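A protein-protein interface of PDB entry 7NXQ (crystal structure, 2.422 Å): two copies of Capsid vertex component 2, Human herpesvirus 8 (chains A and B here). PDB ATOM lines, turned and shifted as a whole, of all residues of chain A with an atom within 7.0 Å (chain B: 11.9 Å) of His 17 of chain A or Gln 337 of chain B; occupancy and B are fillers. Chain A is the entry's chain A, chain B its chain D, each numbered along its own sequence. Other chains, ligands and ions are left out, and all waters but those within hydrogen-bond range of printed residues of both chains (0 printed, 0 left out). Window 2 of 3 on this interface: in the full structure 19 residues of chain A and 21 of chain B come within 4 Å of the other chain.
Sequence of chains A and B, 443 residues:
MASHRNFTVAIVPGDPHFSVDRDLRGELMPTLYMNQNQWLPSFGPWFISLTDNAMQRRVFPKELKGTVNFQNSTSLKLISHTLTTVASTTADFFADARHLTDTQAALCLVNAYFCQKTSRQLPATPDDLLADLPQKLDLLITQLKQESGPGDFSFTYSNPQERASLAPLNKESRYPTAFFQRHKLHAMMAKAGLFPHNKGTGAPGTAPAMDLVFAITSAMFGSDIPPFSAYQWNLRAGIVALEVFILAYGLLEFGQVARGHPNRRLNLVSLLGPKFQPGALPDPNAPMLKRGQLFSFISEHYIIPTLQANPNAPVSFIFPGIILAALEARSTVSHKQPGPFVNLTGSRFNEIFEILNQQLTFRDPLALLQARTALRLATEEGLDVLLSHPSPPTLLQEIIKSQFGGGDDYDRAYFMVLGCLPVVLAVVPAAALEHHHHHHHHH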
ATOM      1  N   THR A   8      30.417  -8.881  32.207  1.00  0.00           N
ATOM      2  CA  THR A   8      30.351  -8.401  30.839  1.00  0.00           C
ATOM      3  C   THR A   8      31.519  -8.912  29.997  1.00  0.00           C
ATOM      4  O   THR A   8      32.647  -8.977  30.481  1.00  0.00           O
ATOM      5  CB  THR A   8      30.286  -6.870  30.879  1.00  0.00           C
ATOM      6  OG1 THR A   8      29.107  -6.485  31.580  1.00  0.00           O
ATOM      7  CG2 THR A   8      30.256  -6.249  29.516  1.00  0.00           C
ATOM      8  N   VAL A   9      31.245  -9.303  28.745  1.00  0.00           N
ATOM      9  CA  VAL A   9      32.274  -9.764  27.809  1.00  0.00           C
ATOM     10  C   VAL A   9      32.099  -9.073  26.442  1.00  0.00           C
ATOM     11  O   VAL A   9      31.014  -8.621  26.109  1.00  0.00           O
ATOM     12  CB  VAL A   9      32.327 -11.308  27.629  1.00  0.00           C
ATOM     13  CG1 VAL A   9      32.690 -12.021  28.920  1.00  0.00           C
ATOM     14  CG2 VAL A   9      31.027 -11.849  27.044  1.00  0.00           C
ATOM     15  N   ALA A  10      33.163  -8.999  25.653  1.00  0.00           N
ATOM     16  CA  ALA A  10      33.119  -8.461  24.296  1.00  0.00           C
ATOM     17  C   ALA A  10      34.036  -9.353  23.467  1.00  0.00           C
ATOM     18  O   ALA A  10      35.102  -9.749  23.933  1.00  0.00           O
ATOM     19  CB  ALA A  10      33.584  -7.018  24.257  1.00  0.00           C
ATOM     20  N   ILE A  11      33.596  -9.726  22.268  1.00  0.00           N
ATOM     21  CA  ILE A  11      34.339 -10.673  21.441  1.00  0.00           C
ATOM     22  C   ILE A  11      35.255  -9.979  20.413  1.00  0.00           C
ATOM     23  O   ILE A  11      36.433 -10.315  20.323  1.00  0.00           O
ATOM     24  CB  ILE A  11      33.386 -11.710  20.790  1.00  0.00           C
ATOM     25  CG1 ILE A  11      32.361 -12.273  21.803  1.00  0.00           C
ATOM     26  CG2 ILE A  11      34.161 -12.823  20.111  1.00  0.00           C
ATOM     27  CD1 ILE A  11      32.927 -12.884  23.032  1.00  0.00           C
ATOM     28  N   ASP A  15      32.019  -4.171  18.329  1.00  0.00           N
ATOM     29  CA  ASP A  15      30.780  -4.903  18.576  1.00  0.00           C
ATOM     30  C   ASP A  15      30.200  -4.610  19.974  1.00  0.00           C
ATOM     31  O   ASP A  15      30.920  -4.077  20.827  1.00  0.00           O
ATOM     32  CB  ASP A  15      31.043  -6.405  18.393  1.00  0.00           C
ATOM     33  CG  ASP A  15      30.414  -6.928  17.133  1.00  0.00           C
ATOM     34  OD1 ASP A  15      30.387  -6.178  16.132  1.00  0.00           O
ATOM     35  OD2 ASP A  15      29.943  -8.085  17.142  1.00  0.00           O
ATOM     36  N   PRO A  16      28.916  -4.951  20.253  1.00  0.00           N
ATOM     37  CA  PRO A  16      28.387  -4.711  21.595  1.00  0.00           C
ATOM     38  C   PRO A  16      28.989  -5.634  22.654  1.00  0.00           C
ATOM     39  O   PRO A  16      29.508  -6.709  22.360  1.00  0.00           O
ATOM     40  CB  PRO A  16      26.892  -4.995  21.430  1.00  0.00           C
ATOM     41  CG  PRO A  16      26.824  -5.979  20.350  1.00  0.00           C
ATOM     42  CD  PRO A  16      27.892  -5.573  19.386  1.00  0.00           C
ATOM     43  N   HIS A  17      28.920  -5.191  23.897  1.00  0.00           N
ATOM     44  CA  HIS A  17      29.332  -5.962  25.055  1.00  0.00           C
ATOM     45  C   HIS A  17      28.100  -6.761  25.505  1.00  0.00           C
ATOM     46  O   HIS A  17      26.978  -6.268  25.412  1.00  0.00           O
ATOM     47  CB  HIS A  17      29.755  -5.006  26.178  1.00  0.00           C
ATOM     48  CG  HIS A  17      31.153  -4.485  26.052  1.00  0.00           C
ATOM     49  ND1 HIS A  17      31.445  -3.370  25.283  1.00  0.00           N
ATOM     50  CD2 HIS A  17      32.294  -4.920  26.643  1.00  0.00           C
ATOM     51  CE1 HIS A  17      32.753  -3.178  25.412  1.00  0.00           C
ATOM     52  NE2 HIS A  17      33.304  -4.087  26.218  1.00  0.00           N
ATOM     53  N   PHE A  18      28.298  -7.977  25.989  1.00  0.00           N
ATOM     54  CA  PHE A  18      27.202  -8.819  26.450  1.00  0.00           C
ATOM     55  C   PHE A  18      27.260  -8.959  27.953  1.00  0.00           C
ATOM     56  O   PHE A  18      28.285  -9.355  28.487  1.00  0.00           O
ATOM     57  CB  PHE A  18      27.269 -10.218  25.813  1.00  0.00           C
ATOM     58  CG  PHE A  18      27.110 -10.251  24.316  1.00  0.00           C
ATOM     59  CD1 PHE A  18      28.212 -10.215  23.489  1.00  0.00           C
ATOM     60  CD2 PHE A  18      25.860 -10.371  23.738  1.00  0.00           C
ATOM     61  CE1 PHE A  18      28.063 -10.273  22.114  1.00  0.00           C
ATOM     62  CE2 PHE A  18      25.715 -10.391  22.361  1.00  0.00           C
ATOM     63  CZ  PHE A  18      26.814 -10.352  21.560  1.00  0.00           C
ATOM     64  N   SER A  19      26.165  -8.643  28.640  1.00  0.00           N
ATOM     65  CA  SER A  19      26.084  -8.823  30.076  1.00  0.00           C
ATOM     66  C   SER A  19      25.365 -10.135  30.309  1.00  0.00           C
ATOM     67  O   SER A  19      24.256 -10.324  29.821  1.00  0.00           O
ATOM     68  CB  SER A  19      25.304  -7.691  30.715  1.00  0.00           C
ATOM     69  OG  SER A  19      26.236  -6.800  31.296  1.00  0.00           O
ATOM     70  N   PHE A 297      42.300  -8.300  22.033  1.00  0.00           N
ATOM     71  CA  PHE A 297      40.965  -7.837  22.368  1.00  0.00           C
ATOM     72  C   PHE A 297      40.173  -8.991  22.995  1.00  0.00           C
ATOM     73  O   PHE A 297      39.555  -8.801  24.041  1.00  0.00           O
ATOM     74  CB  PHE A 297      40.236  -7.291  21.128  1.00  0.00           C
ATOM     75  CG  PHE A 297      38.925  -6.625  21.476  1.00  0.00           C
ATOM     76  CD1 PHE A 297      37.765  -7.369  21.620  1.00  0.00           C
ATOM     77  CD2 PHE A 297      38.857  -5.262  21.684  1.00  0.00           C
ATOM     78  CE1 PHE A 297      36.578  -6.762  21.995  1.00  0.00           C
ATOM     79  CE2 PHE A 297      37.658  -4.659  22.026  1.00  0.00           C
ATOM     80  CZ  PHE A 297      36.525  -5.411  22.174  1.00  0.00           C
ATOM     81  N   HIS A 301      38.897  -8.757  26.831  1.00  0.00           N
ATOM     82  CA  HIS A 301      37.467  -8.562  26.979  1.00  0.00           C
ATOM     83  C   HIS A 301      36.651  -9.836  27.068  1.00  0.00           C
ATOM     84  O   HIS A 301      35.489  -9.757  27.437  1.00  0.00           O
ATOM     85  CB  HIS A 301      36.939  -7.656  25.868  1.00  0.00           C
ATOM     86  CG  HIS A 301      37.637  -6.332  25.841  1.00  0.00           C
ATOM     87  ND1 HIS A 301      37.271  -5.306  26.694  1.00  0.00           N
ATOM     88  CD2 HIS A 301      38.702  -5.933  25.113  1.00  0.00           C
ATOM     89  CE1 HIS A 301      38.100  -4.307  26.436  1.00  0.00           C
ATOM     90  NE2 HIS A 301      38.979  -4.635  25.492  1.00  0.00           N
ATOM     91  N   TYR A 414      33.836 -15.362  16.743  1.00  0.00           N
ATOM     92  CA  TYR A 414      32.566 -15.715  17.367  1.00  0.00           C
ATOM     93  C   TYR A 414      32.328 -17.223  17.408  1.00  0.00           C
ATOM     94  O   TYR A 414      31.752 -17.707  18.365  1.00  0.00           O
ATOM     95  CB  TYR A 414      31.403 -14.994  16.693  1.00  0.00           C
ATOM     96  CG  TYR A 414      31.105 -13.648  17.310  1.00  0.00           C
ATOM     97  CD1 TYR A 414      30.342 -13.543  18.461  1.00  0.00           C
ATOM     98  CD2 TYR A 414      31.533 -12.475  16.707  1.00  0.00           C
ATOM     99  CE1 TYR A 414      30.033 -12.309  19.013  1.00  0.00           C
ATOM    100  CE2 TYR A 414      31.243 -11.236  17.256  1.00  0.00           C
ATOM    101  CZ  TYR A 414      30.485 -11.155  18.407  1.00  0.00           C
ATOM    102  OH  TYR A 414      30.189  -9.926  18.954  1.00  0.00           O
ATOM    103  N   SER B  49      12.734  -8.867  27.057  1.00  0.00           N
ATOM    104  CA  SER B  49      13.853  -9.391  27.848  1.00  0.00           C
ATOM    105  C   SER B  49      13.328 -10.199  29.040  1.00  0.00           C
ATOM    106  O   SER B  49      13.910 -11.226  29.387  1.00  0.00           O
ATOM    107  CB  SER B  49      14.732  -8.255  28.364  1.00  0.00           C
ATOM    108  OG  SER B  49      15.426  -7.615  27.307  1.00  0.00           O
ATOM    109  N   ARG B 330      18.132   1.453  38.761  1.00  0.00           N
ATOM    110  CA  ARG B 330      19.189   0.841  39.574  1.00  0.00           C
ATOM    111  C   ARG B 330      20.273   0.274  38.673  1.00  0.00           C
ATOM    112  O   ARG B 330      21.452   0.389  39.002  1.00  0.00           O
ATOM    113  CB  ARG B 330      18.668  -0.336  40.399  1.00  0.00           C
ATOM    114  CG  ARG B 330      17.569  -0.065  41.374  1.00  0.00           C
ATOM    115  CD  ARG B 330      17.188  -1.390  41.989  1.00  0.00           C
ATOM    116  NE  ARG B 330      16.573  -2.289  41.015  1.00  0.00           N
ATOM    117  CZ  ARG B 330      16.565  -3.611  41.113  1.00  0.00           C
ATOM    118  NH1 ARG B 330      15.965  -4.346  40.186  1.00  0.00           N
ATOM    119  NH2 ARG B 330      17.168  -4.213  42.135  1.00  0.00           N
ATOM    120  N   SER B 331      19.869  -0.382  37.563  1.00  0.00           N
ATOM    121  CA  SER B 331      20.764  -1.023  36.591  1.00  0.00           C
ATOM    122  C   SER B 331      21.734  -0.023  35.954  1.00  0.00           C
ATOM    123  O   SER B 331      22.914  -0.329  35.791  1.00  0.00           O
ATOM    124  CB  SER B 331      19.952  -1.720  35.497  1.00  0.00           C
ATOM    125  OG  SER B 331      18.806  -2.390  36.006  1.00  0.00           O
ATOM    126  N   THR B 332      21.238   1.179  35.621  1.00  0.00           N
ATOM    127  CA  THR B 332      22.023   2.233  34.978  1.00  0.00           C
ATOM    128  C   THR B 332      23.219   2.708  35.836  1.00  0.00           C
ATOM    129  O   THR B 332      23.120   2.823  37.062  1.00  0.00           O
ATOM    130  CB  THR B 332      21.112   3.404  34.536  1.00  0.00           C
ATOM    131  OG1 THR B 332      20.766   4.218  35.662  1.00  0.00           O
ATOM    132  CG2 THR B 332      19.844   2.936  33.805  1.00  0.00           C
ATOM    133  N   LYS B 336      28.128   0.233  33.428  1.00  0.00           N
ATOM    134  CA  LYS B 336      29.448  -0.340  33.687  1.00  0.00           C
ATOM    135  C   LYS B 336      30.443  -0.031  32.555  1.00  0.00           C
ATOM    136  O   LYS B 336      31.555   0.418  32.825  1.00  0.00           O
ATOM    137  CB  LYS B 336      29.343  -1.859  33.934  1.00  0.00           C
ATOM    138  CG  LYS B 336      28.388  -2.232  35.069  1.00  0.00           C
ATOM    139  CD  LYS B 336      28.005  -3.719  35.061  1.00  0.00           C
ATOM    140  CE  LYS B 336      29.028  -4.613  35.729  1.00  0.00           C
ATOM    141  NZ  LYS B 336      28.556  -6.020  35.816  1.00  0.00           N
ATOM    142  N   GLN B 337      30.052  -0.269  31.292  1.00  0.00           N
ATOM    143  CA  GLN B 337      30.920  -0.004  30.141  1.00  0.00           C
ATOM    144  C   GLN B 337      30.198   0.824  29.069  1.00  0.00           C
ATOM    145  O   GLN B 337      29.016   0.604  28.806  1.00  0.00           O
ATOM    146  CB  GLN B 337      31.483  -1.315  29.545  1.00  0.00           C
ATOM    147  CG  GLN B 337      32.572  -1.956  30.401  1.00  0.00           C
ATOM    148  CD  GLN B 337      33.826  -2.292  29.628  1.00  0.00           C
ATOM    149  OE1 GLN B 337      33.808  -2.459  28.405  1.00  0.00           O
ATOM    150  NE2 GLN B 337      34.952  -2.387  30.323  1.00  0.00           N
ATOM    151  N   PRO B 338      30.899   1.778  28.430  1.00  0.00           N
ATOM    152  CA  PRO B 338      30.238   2.610  27.410  1.00  0.00           C
ATOM    153  C   PRO B 338      30.230   2.027  25.987  1.00  0.00           C
ATOM    154  O   PRO B 338      31.221   1.455  25.522  1.00  0.00           O
ATOM    155  CB  PRO B 338      31.008   3.929  27.489  1.00  0.00           C
ATOM    156  CG  PRO B 338      32.389   3.529  27.949  1.00  0.00           C
ATOM    157  CD  PRO B 338      32.302   2.183  28.639  1.00  0.00           C
ATOM    158  N   GLY B 339      29.100   2.205  25.302  1.00  0.00           N
ATOM    159  CA  GLY B 339      28.911   1.741  23.930  1.00  0.00           C
ATOM    160  C   GLY B 339      27.670   0.884  23.751  1.00  0.00           C
ATOM    161  O   GLY B 339      26.780   0.883  24.606  1.00  0.00           O
ATOM    162  N   PRO B 340      27.574   0.146  22.629  1.00  0.00           N
ATOM    163  CA  PRO B 340      26.421  -0.754  22.451  1.00  0.00           C
ATOM    164  C   PRO B 340      26.496  -1.909  23.454  1.00  0.00           C
ATOM    165  O   PRO B 340      27.592  -2.367  23.786  1.00  0.00           O
ATOM    166  CB  PRO B 340      26.549  -1.251  21.001  1.00  0.00           C
ATOM    167  CG  PRO B 340      27.736  -0.543  20.411  1.00  0.00           C
ATOM    168  CD  PRO B 340      28.550   0.021  21.532  1.00  0.00           C
ATOM    169  N   PHE B 341      25.343  -2.363  23.954  1.00  0.00           N
ATOM    170  CA  PHE B 341      25.321  -3.413  24.959  1.00  0.00           C
ATOM    171  C   PHE B 341      24.043  -4.262  24.904  1.00  0.00           C
ATOM    172  O   PHE B 341      22.947  -3.738  24.731  1.00  0.00           O
ATOM    173  CB  PHE B 341      25.577  -2.766  26.329  1.00  0.00           C
ATOM    174  CG  PHE B 341      24.800  -3.189  27.545  1.00  0.00           C
ATOM    175  CD1 PHE B 341      23.549  -2.671  27.796  1.00  0.00           C
ATOM    176  CD2 PHE B 341      25.390  -3.962  28.526  1.00  0.00           C
ATOM    177  CE1 PHE B 341      22.853  -3.017  28.942  1.00  0.00           C
ATOM    178  CE2 PHE B 341      24.695  -4.293  29.685  1.00  0.00           C
ATOM    179  CZ  PHE B 341      23.431  -3.818  29.887  1.00  0.00           C
ATOM    180  N   VAL B 342      24.208  -5.583  25.000  1.00  0.00           N
ATOM    181  CA  VAL B 342      23.132  -6.562  24.989  1.00  0.00           C
ATOM    182  C   VAL B 342      22.998  -7.095  26.405  1.00  0.00           C
ATOM    183  O   VAL B 342      23.939  -7.682  26.922  1.00  0.00           O
ATOM    184  CB  VAL B 342      23.444  -7.717  24.017  1.00  0.00           C
ATOM    185  CG1 VAL B 342      22.285  -8.695  23.943  1.00  0.00           C
ATOM    186  CG2 VAL B 342      23.814  -7.198  22.635  1.00  0.00           C
ATOM    187  N   ASN B 343      21.847  -6.894  27.036  1.00  0.00           N
ATOM    188  CA  ASN B 343      21.626  -7.336  28.403  1.00  0.00           C
ATOM    189  C   ASN B 343      20.919  -8.696  28.488  1.00  0.00           C
ATOM    190  O   ASN B 343      19.705  -8.772  28.349  1.00  0.00           O
ATOM    191  CB  ASN B 343      20.846  -6.277  29.168  1.00  0.00           C
ATOM    192  CG  ASN B 343      20.924  -6.401  30.656  1.00  0.00           C
ATOM    193  OD1 ASN B 343      21.460  -7.362  31.199  1.00  0.00           O
ATOM    194  ND2 ASN B 343      20.388  -5.420  31.354  1.00  0.00           N
ATOM    195  N   LEU B 344      21.682  -9.763  28.759  1.00  0.00           N
ATOM    196  CA  LEU B 344      21.137 -11.113  28.929  1.00  0.00           C
ATOM    197  C   LEU B 344      21.054 -11.528  30.418  1.00  0.00           C
ATOM    198  O   LEU B 344      20.966 -12.724  30.714  1.00  0.00           O
ATOM    199  CB  LEU B 344      21.982 -12.141  28.159  1.00  0.00           C
ATOM    200  CG  LEU B 344      22.216 -11.864  26.691  1.00  0.00           C
ATOM    201  CD1 LEU B 344      23.181 -12.868  26.093  1.00  0.00           C
ATOM    202  CD2 LEU B 344      20.909 -11.850  25.929  1.00  0.00           C
ATOM    203  N   THR B 345      21.096 -10.556  31.349  1.00  0.00           N
ATOM    204  CA  THR B 345      21.027 -10.835  32.782  1.00  0.00           C
ATOM    205  C   THR B 345      19.583 -10.877  33.261  1.00  0.00           C
ATOM    206  O   THR B 345      18.703 -10.279  32.646  1.00  0.00           O
ATOM    207  CB  THR B 345      21.864  -9.821  33.584  1.00  0.00           C
ATOM    208  OG1 THR B 345      21.252  -8.536  33.508  1.00  0.00           O
ATOM    209  CG2 THR B 345      23.287  -9.735  33.113  1.00  0.00           C
ATOM    210  N   ARG B 348      17.427  -7.817  37.054  1.00  0.00           N
ATOM    211  CA  ARG B 348      16.352  -6.822  37.085  1.00  0.00           C
ATOM    212  C   ARG B 348      14.957  -7.428  37.218  1.00  0.00           C
ATOM    213  O   ARG B 348      14.014  -6.711  37.552  1.00  0.00           O
ATOM    214  CB  ARG B 348      16.426  -5.860  35.891  1.00  0.00           C
ATOM    215  CG  ARG B 348      16.746  -6.524  34.578  1.00  0.00           C
ATOM    216  CD  ARG B 348      17.158  -5.486  33.568  1.00  0.00           C
ATOM    217  NE  ARG B 348      17.190  -6.053  32.222  1.00  0.00           N
ATOM    218  CZ  ARG B 348      16.874  -5.384  31.119  1.00  0.00           C
ATOM    219  NH1 ARG B 348      16.513  -4.112  31.187  1.00  0.00           N
ATOM    220  NH2 ARG B 348      16.940  -5.976  29.937  1.00  0.00           N
ATOM    221  N   GLU B 398      14.562   8.797  28.974  1.00  0.00           N
ATOM    222  CA  GLU B 398      15.515   7.867  28.388  1.00  0.00           C
ATOM    223  C   GLU B 398      15.121   6.421  28.708  1.00  0.00           C
ATOM    224  O   GLU B 398      15.138   5.583  27.816  1.00  0.00           O
ATOM    225  CB  GLU B 398      16.940   8.208  28.873  1.00  0.00           C
ATOM    226  CG  GLU B 398      17.958   7.080  28.839  1.00  0.00           C
ATOM    227  CD  GLU B 398      18.300   6.545  27.463  1.00  0.00           C
ATOM    228  OE1 GLU B 398      18.374   7.347  26.504  1.00  0.00           O
ATOM    229  OE2 GLU B 398      18.503   5.314  27.346  1.00  0.00           O
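No residue of chain B comes within 4 Å of Val 9 of chain A.
No residue of chain B comes within 4 Å of Ala 10 of chain A.
His 17 of chain A touches just these residues of chain B: Gln 337, Pro 340, Phe 341 and Val 342.
Of chain B, only Val 342 comes within 4 Å of Phe 18 of chain A.
Of chain B, only Phe 341, Val 342, Asn 343, Leu 344 and Thr 345 come within 4 Å of Ser 19 of chain A.
Gln 337 of chain B touches just one residue of chain A: His 17.
Printed residues of chain A within 4 Å of Pro 340 of chain B: Pro 16 (3.3 Å) and His 17 (3.1 Å).
Of the printed residues of chain A, Phe 341 of chain B touches Pro 16 (3.96 Å), His 17 (3.3 Å) and Ser 19 (3.4 Å).
Of the printed residues of chain A, Val 342 of chain B touches Pro 16 (3.97 Å), His 17 (2.9 Å), Phe 18 (3.5 Å) and Ser 19 (3.0 Å).
Of the printed residues of chain A, Asn 343 of chain B touches Ser 19 (3.9 Å).
The nearest residue of chain B that does not touch His 17 of chain A is Pro 338 of chain B (4.8 Å).
The nearest residue of chain A that does not touch Gln 337 of chain B is His 301 of chain A (4.8 Å).
The nearest printed residue of chain A that does not touch Pro 340 of chain B is Asp 15 of chain A (4.8 Å).
O of Ser 19 of chain A is in hydrogen-bond range of N of Leu 344 of chain B, 2.8 Å away.
The backbone NH of His 17 of chain A lies within hydrogen-bond range of the backbone carbonyl oxygen of Pro 340 of chain B (3.1 Å).
The backbone carbonyl oxygen (O) of Val 342 of chain B lies within hydrogen-bond range of the backbone NH (N) of Ser 19 of chain A.
N of Val 342 of chain B sits at hydrogen-bond distance from O of His 17 of chain A.
NE2 of His 17 of chain A is in hydrogen-bond range of OE1 of Gln 337 of chain B (2.8 Å).
Among the printed residues, merely in contact across the chains: Pro 16 of chain A with Pro 340 of chain B (3.3 Å), His 17 of chain A with Phe 341 of chain B (3.3 Å), Ser 19 of chain A with Phe 341 of chain B (3.4 Å), Ser 19 of chain A with Thr 345 of chain B (3.5 Å), Phe 18 of chain A with Val 342 of chain B (3.5 Å), Ser 19 of chain A with Asn 343 of chain B (3.9 Å), Pro 16 of chain A with Phe 341 of chain B (3.96 Å) and Pro 16 of chain A with Val 342 of chain B (3.97 Å).
Hydrophobic or aromatic side chains of chain B within 4 Å of the printed part of chain A: Pro 340, Phe 341, Val 342 and Leu 344.
Along chain B the printed residues that touch a printed residue of chain A span positions 337 to 345.
Of the 12 printed residues of chain A, 4 touch a printed residue of chain B.
Hydrophobic or aromatic side chains of chain A that line the printed part of chain B: Pro 16, His 17 and Phe 18.
Among the printed residues, 13 pairs touch across the chains.
Among the printed residues, no Asp or Glu carboxylate lies within 4 Å of a Lys or Arg side-chain nitrogen of the other chain.
OG1 of Thr 8 of chain A sits at hydrogen-bond distance from OG of Ser 19 of chain A (2.9 Å).
The backbone carbonyl oxygen (O) of Val 9 of chain A lies within hydrogen-bond range of the backbone NH (N) of Phe 18 of chain A, at 2.8 Å.
The side-chain amide nitrogen of Asn 343 of chain B lies close to the guanidinium group of Arg 348 of chain B, at 3.4 Å.
The side-chain amide oxygen (OD1) of Asn 343 of chain B lies within hydrogen-bond range of the side-chain hydroxyl (OG1) of Thr 345 of chain B (2.6 Å).
No position is printed for both chains.
Of the 13 pairs that touch across the chains among the printed residues, none has its exchanged pair printed and touching as well.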
